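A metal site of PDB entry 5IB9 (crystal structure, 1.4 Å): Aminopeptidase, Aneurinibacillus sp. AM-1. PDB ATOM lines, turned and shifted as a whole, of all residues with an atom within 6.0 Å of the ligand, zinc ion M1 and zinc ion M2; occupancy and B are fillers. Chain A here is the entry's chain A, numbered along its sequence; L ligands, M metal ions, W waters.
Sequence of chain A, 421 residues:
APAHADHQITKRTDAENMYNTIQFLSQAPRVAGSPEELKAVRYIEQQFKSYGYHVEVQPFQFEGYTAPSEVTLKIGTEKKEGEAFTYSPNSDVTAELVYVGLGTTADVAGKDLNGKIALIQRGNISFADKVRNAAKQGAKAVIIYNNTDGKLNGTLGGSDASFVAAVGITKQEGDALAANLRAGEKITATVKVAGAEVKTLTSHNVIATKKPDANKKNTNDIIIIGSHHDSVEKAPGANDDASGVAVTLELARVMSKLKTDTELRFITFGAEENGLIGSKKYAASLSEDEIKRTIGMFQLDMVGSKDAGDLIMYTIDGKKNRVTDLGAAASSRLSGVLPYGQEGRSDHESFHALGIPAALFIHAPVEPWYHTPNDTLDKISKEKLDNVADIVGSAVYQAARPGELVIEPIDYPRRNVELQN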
ATOM      1  N   HIS A 228      -2.599   2.160   7.385  1.00  0.00           N
ATOM      2  CA  HIS A 228      -1.559   3.138   6.985  1.00  0.00           C
ATOM      3  C   HIS A 228      -1.918   3.848   5.690  1.00  0.00           C
ATOM      4  O   HIS A 228      -2.555   3.248   4.796  1.00  0.00           O
ATOM      5  CB  HIS A 228      -0.118   2.474   6.868  1.00  0.00           C
ATOM      6  CG  HIS A 228       0.043   1.451   5.748  1.00  0.00           C
ATOM      7  ND1 HIS A 228       0.575   1.820   4.501  1.00  0.00           N
ATOM      8  CD2 HIS A 228      -0.068   0.124   5.773  1.00  0.00           C
ATOM      9  CE1 HIS A 228       0.677   0.675   3.777  1.00  0.00           C
ATOM     10  NE2 HIS A 228       0.271  -0.338   4.513  1.00  0.00           N
ATOM     11  N   ASP A 230       0.273   5.685   3.657  1.00  0.00           N
ATOM     12  CA  ASP A 230       1.323   5.800   2.608  1.00  0.00           C
ATOM     13  C   ASP A 230       1.340   4.533   1.742  1.00  0.00           C
ATOM     14  O   ASP A 230       0.815   3.467   2.121  1.00  0.00           O
ATOM     15  CB  ASP A 230       2.697   5.966   3.245  1.00  0.00           C
ATOM     16  CG  ASP A 230       3.156   4.787   4.079  1.00  0.00           C
ATOM     17  OD1 ASP A 230       2.380   4.216   4.914  1.00  0.00           O
ATOM     18  OD2 ASP A 230       4.334   4.393   3.906  1.00  0.00           O
ATOM     19  N   VAL A 232       4.015   2.489  -1.439  1.00  0.00           N
ATOM     20  CA  VAL A 232       5.413   2.502  -1.997  1.00  0.00           C
ATOM     21  C   VAL A 232       5.507   3.322  -3.290  1.00  0.00           C
ATOM     22  O   VAL A 232       4.500   3.596  -3.956  1.00  0.00           O
ATOM     23  CB  VAL A 232       5.891   1.058  -2.260  1.00  0.00           C
ATOM     24  CG1 VAL A 232       5.940   0.279  -0.898  1.00  0.00           C
ATOM     25  CG2 VAL A 232       5.099   0.315  -3.337  1.00  0.00           C
ATOM     26  N   ASP A 240      -3.078  -1.493  -0.999  1.00  0.00           N
ATOM     27  CA  ASP A 240      -2.012  -1.372  -0.003  1.00  0.00           C
ATOM     28  C   ASP A 240      -1.740   0.118   0.154  1.00  0.00           C
ATOM     29  O   ASP A 240      -0.843   0.612  -0.520  1.00  0.00           O
ATOM     30  CB  ASP A 240      -0.678  -2.133  -0.444  1.00  0.00           C
ATOM     31  CG  ASP A 240       0.342  -2.258   0.630  1.00  0.00           C
ATOM     32  OD1 ASP A 240      -0.144  -1.823   1.855  1.00  0.00           O
ATOM     33  OD2 ASP A 240       1.612  -2.573   0.591  1.00  0.00           O
ATOM     34  N   ASP A 241      -2.396   0.936   1.022  1.00  0.00           N
ATOM     35  CA  ASP A 241      -3.363   0.458   1.981  1.00  0.00           C
ATOM     36  C   ASP A 241      -4.498   1.454   2.006  1.00  0.00           C
ATOM     37  O   ASP A 241      -5.114   1.675   3.055  1.00  0.00           O
ATOM     38  CB  ASP A 241      -2.767   0.251   3.378  1.00  0.00           C
ATOM     39  CG  ASP A 241      -3.757  -0.472   4.278  1.00  0.00           C
ATOM     40  OD1 ASP A 241      -4.704  -1.177   3.865  1.00  0.00           O
ATOM     41  OD2 ASP A 241      -3.577  -0.277   5.583  1.00  0.00           O
ATOM     42  N   GLU A 272       4.520   3.724   7.031  1.00  0.00           N
ATOM     43  CA  GLU A 272       4.472   2.286   7.267  1.00  0.00           C
ATOM     44  C   GLU A 272       5.495   1.552   6.377  1.00  0.00           C
ATOM     45  O   GLU A 272       6.177   0.633   6.864  1.00  0.00           O
ATOM     46  CB  GLU A 272       3.037   1.718   7.127  1.00  0.00           C
ATOM     47  CG  GLU A 272       2.922   0.252   7.579  1.00  0.00           C
ATOM     48  CD  GLU A 272       3.164  -0.744   6.420  1.00  0.00           C
ATOM     49  OE1 GLU A 272       3.331  -0.334   5.239  1.00  0.00           O
ATOM     50  OE2 GLU A 272       3.179  -1.927   6.830  1.00  0.00           O
ATOM     51  N   GLU A 273       5.556   2.027   5.136  1.00  0.00           N
ATOM     52  CA  GLU A 273       6.354   1.236   4.153  1.00  0.00           C
ATOM     53  C   GLU A 273       7.840   1.445   4.398  1.00  0.00           C
ATOM     54  O   GLU A 273       8.651   0.626   3.881  1.00  0.00           O
ATOM     55  CB  GLU A 273       5.967   1.713   2.781  1.00  0.00           C
ATOM     56  CG  GLU A 273       4.490   1.456   2.291  1.00  0.00           C
ATOM     57  CD  GLU A 273       4.136  -0.030   2.068  1.00  0.00           C
ATOM     58  OE1 GLU A 273       5.007  -0.906   2.402  1.00  0.00           O
ATOM     59  OE2 GLU A 273       2.932  -0.267   1.596  1.00  0.00           O
ATOM     60  N   ASN A 274       8.184   2.439   5.176  1.00  0.00           N
ATOM     61  CA  ASN A 274       9.539   2.744   5.576  1.00  0.00           C
ATOM     62  C   ASN A 274      10.036   1.999   6.795  1.00  0.00           C
ATOM     63  O   ASN A 274      11.108   2.321   7.315  1.00  0.00           O
ATOM     64  CB  ASN A 274       9.674   4.300   5.899  1.00  0.00           C
ATOM     65  CG  ASN A 274       9.190   5.178   4.744  1.00  0.00           C
ATOM     66  OD1 ASN A 274       9.990   5.647   3.910  1.00  0.00           O
ATOM     67  ND2 ASN A 274       7.884   5.260   4.600  1.00  0.00           N
ATOM     68  N   GLY A 275       9.243   1.062   7.352  1.00  0.00           N
ATOM     69  CA  GLY A 275       9.593   0.364   8.534  1.00  0.00           C
ATOM     70  C   GLY A 275       8.713   0.690   9.736  1.00  0.00           C
ATOM     71  O   GLY A 275       9.156   0.695  10.868  1.00  0.00           O
ATOM     72  N   LEU A 276       7.411   0.844   9.491  1.00  0.00           N
ATOM     73  CA  LEU A 276       6.429   1.033  10.578  1.00  0.00           C
ATOM     74  C   LEU A 276       6.692   2.315  11.318  1.00  0.00           C
ATOM     75  O   LEU A 276       6.494   2.313  12.541  1.00  0.00           O
ATOM     76  CB  LEU A 276       6.311  -0.214  11.514  1.00  0.00           C
ATOM     77  CG  LEU A 276       6.320  -1.560  10.772  1.00  0.00           C
ATOM     78  CD1 LEU A 276       6.192  -2.624  11.871  1.00  0.00           C
ATOM     79  CD2 LEU A 276       5.253  -1.714   9.720  1.00  0.00           C
ATOM     80  N   ASP A 301      -4.921  -3.935   6.735  1.00  0.00           N
ATOM     81  CA  ASP A 301      -3.908  -3.673   5.618  1.00  0.00           C
ATOM     82  C   ASP A 301      -4.198  -4.721   4.547  1.00  0.00           C
ATOM     83  O   ASP A 301      -4.058  -5.924   4.811  1.00  0.00           O
ATOM     84  CB  ASP A 301      -2.556  -3.889   6.225  1.00  0.00           C
ATOM     85  CG  ASP A 301      -1.382  -3.265   5.384  1.00  0.00           C
ATOM     86  OD1 ASP A 301      -1.647  -2.854   4.249  1.00  0.00           O
ATOM     87  OD2 ASP A 301      -0.249  -3.047   5.860  1.00  0.00           O
ATOM     88  N   MET A 302      -4.529  -4.217   3.370  1.00  0.00           N
ATOM     89  CA  MET A 302      -4.909  -4.997   2.199  1.00  0.00           C
ATOM     90  C   MET A 302      -6.169  -5.804   2.398  1.00  0.00           C
ATOM     91  O   MET A 302      -6.112  -6.982   2.578  1.00  0.00           O
ATOM     92  CB  MET A 302      -3.724  -5.827   1.754  1.00  0.00           C
ATOM     93  CG  MET A 302      -2.686  -4.955   1.291  1.00  0.00           C
ATOM     94  SD  MET A 302      -1.061  -5.692   0.883  1.00  0.00           S
ATOM     95  CE  MET A 302      -1.526  -6.917  -0.313  1.00  0.00           C
ATOM     96  N   TYR A 314      -3.522 -12.215  11.320  1.00  0.00           N
ATOM     97  CA  TYR A 314      -2.153 -12.587  11.625  1.00  0.00           C
ATOM     98  C   TYR A 314      -1.705 -11.941  12.928  1.00  0.00           C
ATOM     99  O   TYR A 314      -1.934 -10.754  13.200  1.00  0.00           O
ATOM    100  CB  TYR A 314      -1.219 -12.069  10.553  1.00  0.00           C
ATOM    101  CG  TYR A 314      -1.173 -12.901   9.280  1.00  0.00           C
ATOM    102  CD1 TYR A 314      -1.033 -14.265   9.314  1.00  0.00           C
ATOM    103  CD2 TYR A 314      -1.310 -12.269   8.066  1.00  0.00           C
ATOM    104  CE1 TYR A 314      -1.021 -15.002   8.075  1.00  0.00           C
ATOM    105  CE2 TYR A 314      -1.288 -13.010   6.801  1.00  0.00           C
ATOM    106  CZ  TYR A 314      -1.104 -14.345   6.863  1.00  0.00           C
ATOM    107  OH  TYR A 314      -1.119 -15.114   5.695  1.00  0.00           O
ATOM    108  N   GLU A 343       2.267 -13.561  11.288  1.00  0.00           N
ATOM    109  CA  GLU A 343       2.943 -12.697  10.391  1.00  0.00           C
ATOM    110  C   GLU A 343       3.035 -11.311  11.046  1.00  0.00           C
ATOM    111  O   GLU A 343       2.132 -10.900  11.793  1.00  0.00           O
ATOM    112  CB  GLU A 343       2.220 -12.597   9.042  1.00  0.00           C
ATOM    113  CG  GLU A 343       2.906 -11.749   8.044  1.00  0.00           C
ATOM    114  CD  GLU A 343       4.331 -12.223   7.684  1.00  0.00           C
ATOM    115  OE1 GLU A 343       4.405 -12.903   6.610  1.00  0.00           O
ATOM    116  OE2 GLU A 343       5.300 -11.886   8.438  1.00  0.00           O
ATOM    117  N   GLY A 344       4.091 -10.631  10.696  1.00  0.00           N
ATOM    118  CA  GLY A 344       4.378  -9.237  11.106  1.00  0.00           C
ATOM    119  C   GLY A 344       4.116  -8.336   9.869  1.00  0.00           C
ATOM    120  O   GLY A 344       3.110  -8.493   9.159  1.00  0.00           O
ATOM    121  N   ARG A 345       5.052  -7.439   9.608  1.00  0.00           N
ATOM    122  CA  ARG A 345       5.118  -6.662   8.364  1.00  0.00           C
ATOM    123  C   ARG A 345       4.048  -5.584   8.265  1.00  0.00           C
ATOM    124  O   ARG A 345       3.713  -5.140   7.127  1.00  0.00           O
ATOM    125  CB  ARG A 345       5.051  -7.532   7.065  1.00  0.00           C
ATOM    126  CG  ARG A 345       6.114  -8.643   6.981  1.00  0.00           C
ATOM    127  CD  ARG A 345       5.769  -9.685   5.824  1.00  0.00           C
ATOM    128  NE  ARG A 345       5.744  -9.059   4.501  1.00  0.00           N
ATOM    129  CZ  ARG A 345       5.471  -9.694   3.369  1.00  0.00           C
ATOM    130  NH1 ARG A 345       5.244 -11.007   3.374  1.00  0.00           N
ATOM    131  NH2 ARG A 345       5.452  -9.025   2.221  1.00  0.00           N
ATOM    132  N   SER A 346       3.410  -5.229   9.401  1.00  0.00           N
ATOM    133  CA  SER A 346       2.391  -4.092   9.353  1.00  0.00           C
ATOM    134  C   SER A 346       2.341  -3.529  10.772  1.00  0.00           C
ATOM    135  O   SER A 346       3.030  -3.973  11.647  1.00  0.00           O
ATOM    136  CB  SER A 346       1.032  -4.554   8.819  1.00  0.00           C
ATOM    137  OG  SER A 346       0.259  -3.427   8.443  1.00  0.00           O
ATOM    138  N   GLU A 349       2.592  -4.825  14.602  1.00  0.00           N
ATOM    139  CA  GLU A 349       3.882  -5.125  15.288  1.00  0.00           C
ATOM    140  C   GLU A 349       4.276  -4.069  16.278  1.00  0.00           C
ATOM    141  O   GLU A 349       4.974  -4.367  17.251  1.00  0.00           O
ATOM    142  CB  GLU A 349       4.937  -5.222  14.226  1.00  0.00           C
ATOM    143  CG  GLU A 349       6.254  -5.900  14.723  1.00  0.00           C
ATOM    144  CD  GLU A 349       7.123  -6.276  13.509  1.00  0.00           C
ATOM    145  OE1 GLU A 349       6.688  -6.972  12.550  1.00  0.00           O
ATOM    146  OE2 GLU A 349       8.246  -5.832  13.507  1.00  0.00           O
ATOM    147  N   LEU A 360      -3.415  -8.329  12.557  1.00  0.00           N
ATOM    148  CA  LEU A 360      -3.585  -7.805  11.182  1.00  0.00           C
ATOM    149  C   LEU A 360      -4.663  -8.599  10.520  1.00  0.00           C
ATOM    150  O   LEU A 360      -4.667  -9.866  10.510  1.00  0.00           O
ATOM    151  CB  LEU A 360      -2.251  -7.983  10.479  1.00  0.00           C
ATOM    152  CG  LEU A 360      -2.357  -7.859   8.964  1.00  0.00           C
ATOM    153  CD1 LEU A 360      -2.825  -6.442   8.448  1.00  0.00           C
ATOM    154  CD2 LEU A 360      -0.940  -8.200   8.288  1.00  0.00           C
ATOM    155  N   ILE A 362      -6.197  -9.173   6.756  1.00  0.00           N
ATOM    156  CA  ILE A 362      -5.657  -9.051   5.363  1.00  0.00           C
ATOM    157  C   ILE A 362      -6.203 -10.223   4.590  1.00  0.00           C
ATOM    158  O   ILE A 362      -6.538 -11.272   5.199  1.00  0.00           O
ATOM    159  CB  ILE A 362      -4.142  -9.138   5.416  1.00  0.00           C
ATOM    160  CG1 ILE A 362      -3.546  -8.981   3.995  1.00  0.00           C
ATOM    161  CG2 ILE A 362      -3.611 -10.372   6.164  1.00  0.00           C
ATOM    162  CD1 ILE A 362      -2.016  -8.580   4.060  1.00  0.00           C
ATOM    163  N   VAL A 366      -1.906 -12.857  -0.938  1.00  0.00           N
ATOM    164  CA  VAL A 366      -2.102 -11.525  -1.468  1.00  0.00           C
ATOM    165  C   VAL A 366      -2.101 -11.560  -3.008  1.00  0.00           C
ATOM    166  O   VAL A 366      -1.565 -12.483  -3.647  1.00  0.00           O
ATOM    167  CB  VAL A 366      -1.097 -10.480  -0.989  1.00  0.00           C
ATOM    168  CG1 VAL A 366      -1.061 -10.445   0.612  1.00  0.00           C
ATOM    169  CG2 VAL A 366       0.328 -10.675  -1.567  1.00  0.00           C
ATOM    170  N   TYR A 370       0.424  -6.240  -5.519  1.00  0.00           N
ATOM    171  CA  TYR A 370       1.034  -5.721  -4.354  1.00  0.00           C
ATOM    172  C   TYR A 370       2.370  -4.982  -4.643  1.00  0.00           C
ATOM    173  O   TYR A 370       3.231  -5.576  -5.242  1.00  0.00           O
ATOM    174  CB  TYR A 370       1.255  -7.004  -3.527  1.00  0.00           C
ATOM    175  CG  TYR A 370       2.109  -6.822  -2.327  1.00  0.00           C
ATOM    176  CD1 TYR A 370       1.774  -5.926  -1.369  1.00  0.00           C
ATOM    177  CD2 TYR A 370       3.252  -7.608  -2.141  1.00  0.00           C
ATOM    178  CE1 TYR A 370       2.558  -5.745  -0.229  1.00  0.00           C
ATOM    179  CE2 TYR A 370       4.044  -7.451  -1.017  1.00  0.00           C
ATOM    180  CZ  TYR A 370       3.690  -6.486  -0.076  1.00  0.00           C
ATOM    181  OH  TYR A 370       4.477  -6.317   1.051  1.00  0.00           O
ATOM    182  N   HIS A 371       2.536  -3.707  -4.274  1.00  0.00           N
ATOM    183  CA  HIS A 371       3.746  -2.936  -4.426  1.00  0.00           C
ATOM    184  C   HIS A 371       4.073  -2.643  -5.893  1.00  0.00           C
ATOM    185  O   HIS A 371       5.190  -2.254  -6.167  1.00  0.00           O
ATOM    186  CB  HIS A 371       4.914  -3.511  -3.658  1.00  0.00           C
ATOM    187  CG  HIS A 371       4.796  -3.303  -2.154  1.00  0.00           C
ATOM    188  ND1 HIS A 371       5.796  -3.645  -1.288  1.00  0.00           N
ATOM    189  CD2 HIS A 371       3.751  -2.858  -1.392  1.00  0.00           C
ATOM    190  CE1 HIS A 371       5.397  -3.373  -0.026  1.00  0.00           C
ATOM    191  NE2 HIS A 371       4.152  -2.931  -0.080  1.00  0.00           N
HETATM  192  N1  LIG L   1       0.812  -4.747   3.644  1.00  0.00           N
HETATM  193  C1  LIG L   1       2.255  -4.948   3.692  1.00  0.00           C
HETATM  194  C2  LIG L   1       2.541  -6.177   4.553  1.00  0.00           C
HETATM  195  C3  LIG L   1       2.141  -7.548   4.017  1.00  0.00           C
HETATM  196  C4  LIG L   1       2.287  -7.920   2.657  1.00  0.00           C
HETATM  197  C5  LIG L   1       1.650  -8.501   4.941  1.00  0.00           C
HETATM  198  C6  LIG L   1       1.939  -9.222   2.247  1.00  0.00           C
HETATM  199  C7  LIG L   1       1.287  -9.808   4.526  1.00  0.00           C
HETATM  200  C8  LIG L   1       1.430 -10.158   3.169  1.00  0.00           C
HETATM  201  C9  LIG L   1       2.946  -3.709   4.245  1.00  0.00           C
HETATM  202  O1  LIG L   1       2.302  -2.670   3.510  1.00  0.00           O
HETATM  203  C10 LIG L   1       4.374  -3.829   3.834  1.00  0.00           C
HETATM  204  O2  LIG L   1       4.634  -3.772   2.636  1.00  0.00           O
HETATM  205  N2  LIG L   1       5.247  -4.067   4.748  1.00  0.00           N
HETATM  206  C11 LIG L   1       6.653  -4.273   4.379  1.00  0.00           C
HETATM  207  C12 LIG L   1       7.336  -4.508   5.708  1.00  0.00           C
HETATM  208  C13 LIG L   1       7.291  -3.315   6.674  1.00  0.00           C
HETATM  209  C14 LIG L   1       8.145  -3.742   7.854  1.00  0.00           C
HETATM  210  C15 LIG L   1       7.743  -1.978   6.071  1.00  0.00           C
HETATM  211  C16 LIG L   1       6.889  -5.555   3.591  1.00  0.00           C
HETATM  212  O3  LIG L   1       7.960  -5.671   2.939  1.00  0.00           O
HETATM  213  O4  LIG L   1       6.065  -6.492   3.580  1.00  0.00           O
HETATM  214 ZN    ZN M   1       3.057  -2.372   1.570  1.00  0.00          ZN
HETATM  215 ZN    ZN M   2       0.307  -2.228   3.770  1.00  0.00          ZN
HETATM  216  O   HOH W   1       9.034  -8.252   4.858  1.00  0.00           O
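A nitrogen (N2) of the ligand lies close to the backbone carbonyl oxygen (O) of Arg 345 (3.0 Å). An oxygen (O4) of the ligand lies within salt-bridge range of the guanidinium group (NE) of Arg 345 (2.7 Å). The side-chain hydroxyl (OH) of Tyr 370 is in hydrogen-bond range of an oxygen (O4) of the ligand, 3.0 Å away. The side-chain sulfur (SD) of Met 302 lies close to a nitrogen (N1) of the ligand, 3.5 Å away. The side-chain carboxylate (OE1) of Glu 272 lies close to an oxygen (O1) of the ligand.
NH2 of Arg 345 lies within hydrogen-bond range of OH of Tyr 370 (3.1 Å). NE2 of His 228 sits close to OE1 of Glu 272 (3.1 Å). OE1 of Glu 343 is in salt-bridge range of NH1 of Arg 345. The side-chain carboxylate of Glu 349 sits at hydrogen-bond distance from the backbone NH of Arg 345 (3.4 Å). OG of Ser 346 sits close to OD2 of Asp 301 (2.7 Å). The backbone NH (N) of Glu 272 lies within hydrogen-bond range of the side-chain carboxylate (OD1) of Asp 230. The backbone NH (N) of His 228 lies within hydrogen-bond range of the side-chain carboxylate (OD2) of Asp 241 (3.2 Å). N of Met 302 lies within hydrogen-bond range of OD1 of Asp 241 (3.1 Å).
Gly 275 touches the ligand. Leu 276 touches the ligand. Ile 362 touches the ligand. CG1 of Val 366 touches C8 of the ligand, at 3.6 Å. Hydrophobic or aromatic side chains that line the ligand: His 228, Leu 276, Met 302, Ile 362, Val 366, Tyr 370 and His 371. 13 residues have an atom within 4 Å of the ligand: His 228, Asp 240, Glu 272, Glu 273, Gly 275, Leu 276, Asp 301, Met 302, Arg 345, Ile 362, Val 366, Tyr 370 and His 371. Along chain A the residues within 4 Å of the ligand span positions 228 to 371.
Tyr 370 touches zinc ion M1. Of the 23 residues printed, 4 come within 4 Å of zinc ion M1. The nearest printed residue that does not touch zinc ion M1 is Glu 272 (4.2 Å).
Asp 241 touches zinc ion M2. OE1 of Glu 272 touches zinc ion M2, at 3.9 Å. Of the 23 residues printed, 6 come within 4 Å of zinc ion M2.
OD2 of Asp 240 is bound to zinc ion M1 (1.8 Å). NE2 of His 371 binds zinc ion M1, 2.1 Å away. An oxygen (O1) of the ligand is bound to zinc ion M1, at 2.1 Å. OE2 of Glu 273 binds zinc ion M1 (2.1 Å). Zinc ion M1 is bound by O2 of the ligand (2.4 Å). OE1 of Glu 273 binds zinc ion M1 (2.6 Å).
Zinc ion M2 is bound by the side-chain carboxylate (OD1) of Asp 240 (2.0 Å), a ring nitrogen (NE2) of His 228 (2.0 Å), an oxygen (O1) of the ligand (2.1 Å), the side-chain carboxylate (OD1) of Asp 301 (2.1 Å), the side-chain carboxylate (OD2) of Asp 301 (2.3 Å) and a nitrogen (N1) of the ligand (2.6 Å).
Water W1 lies within hydrogen-bond range of O3 of the ligand (3.4 Å) and NE of Arg 345 (3.4 Å).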
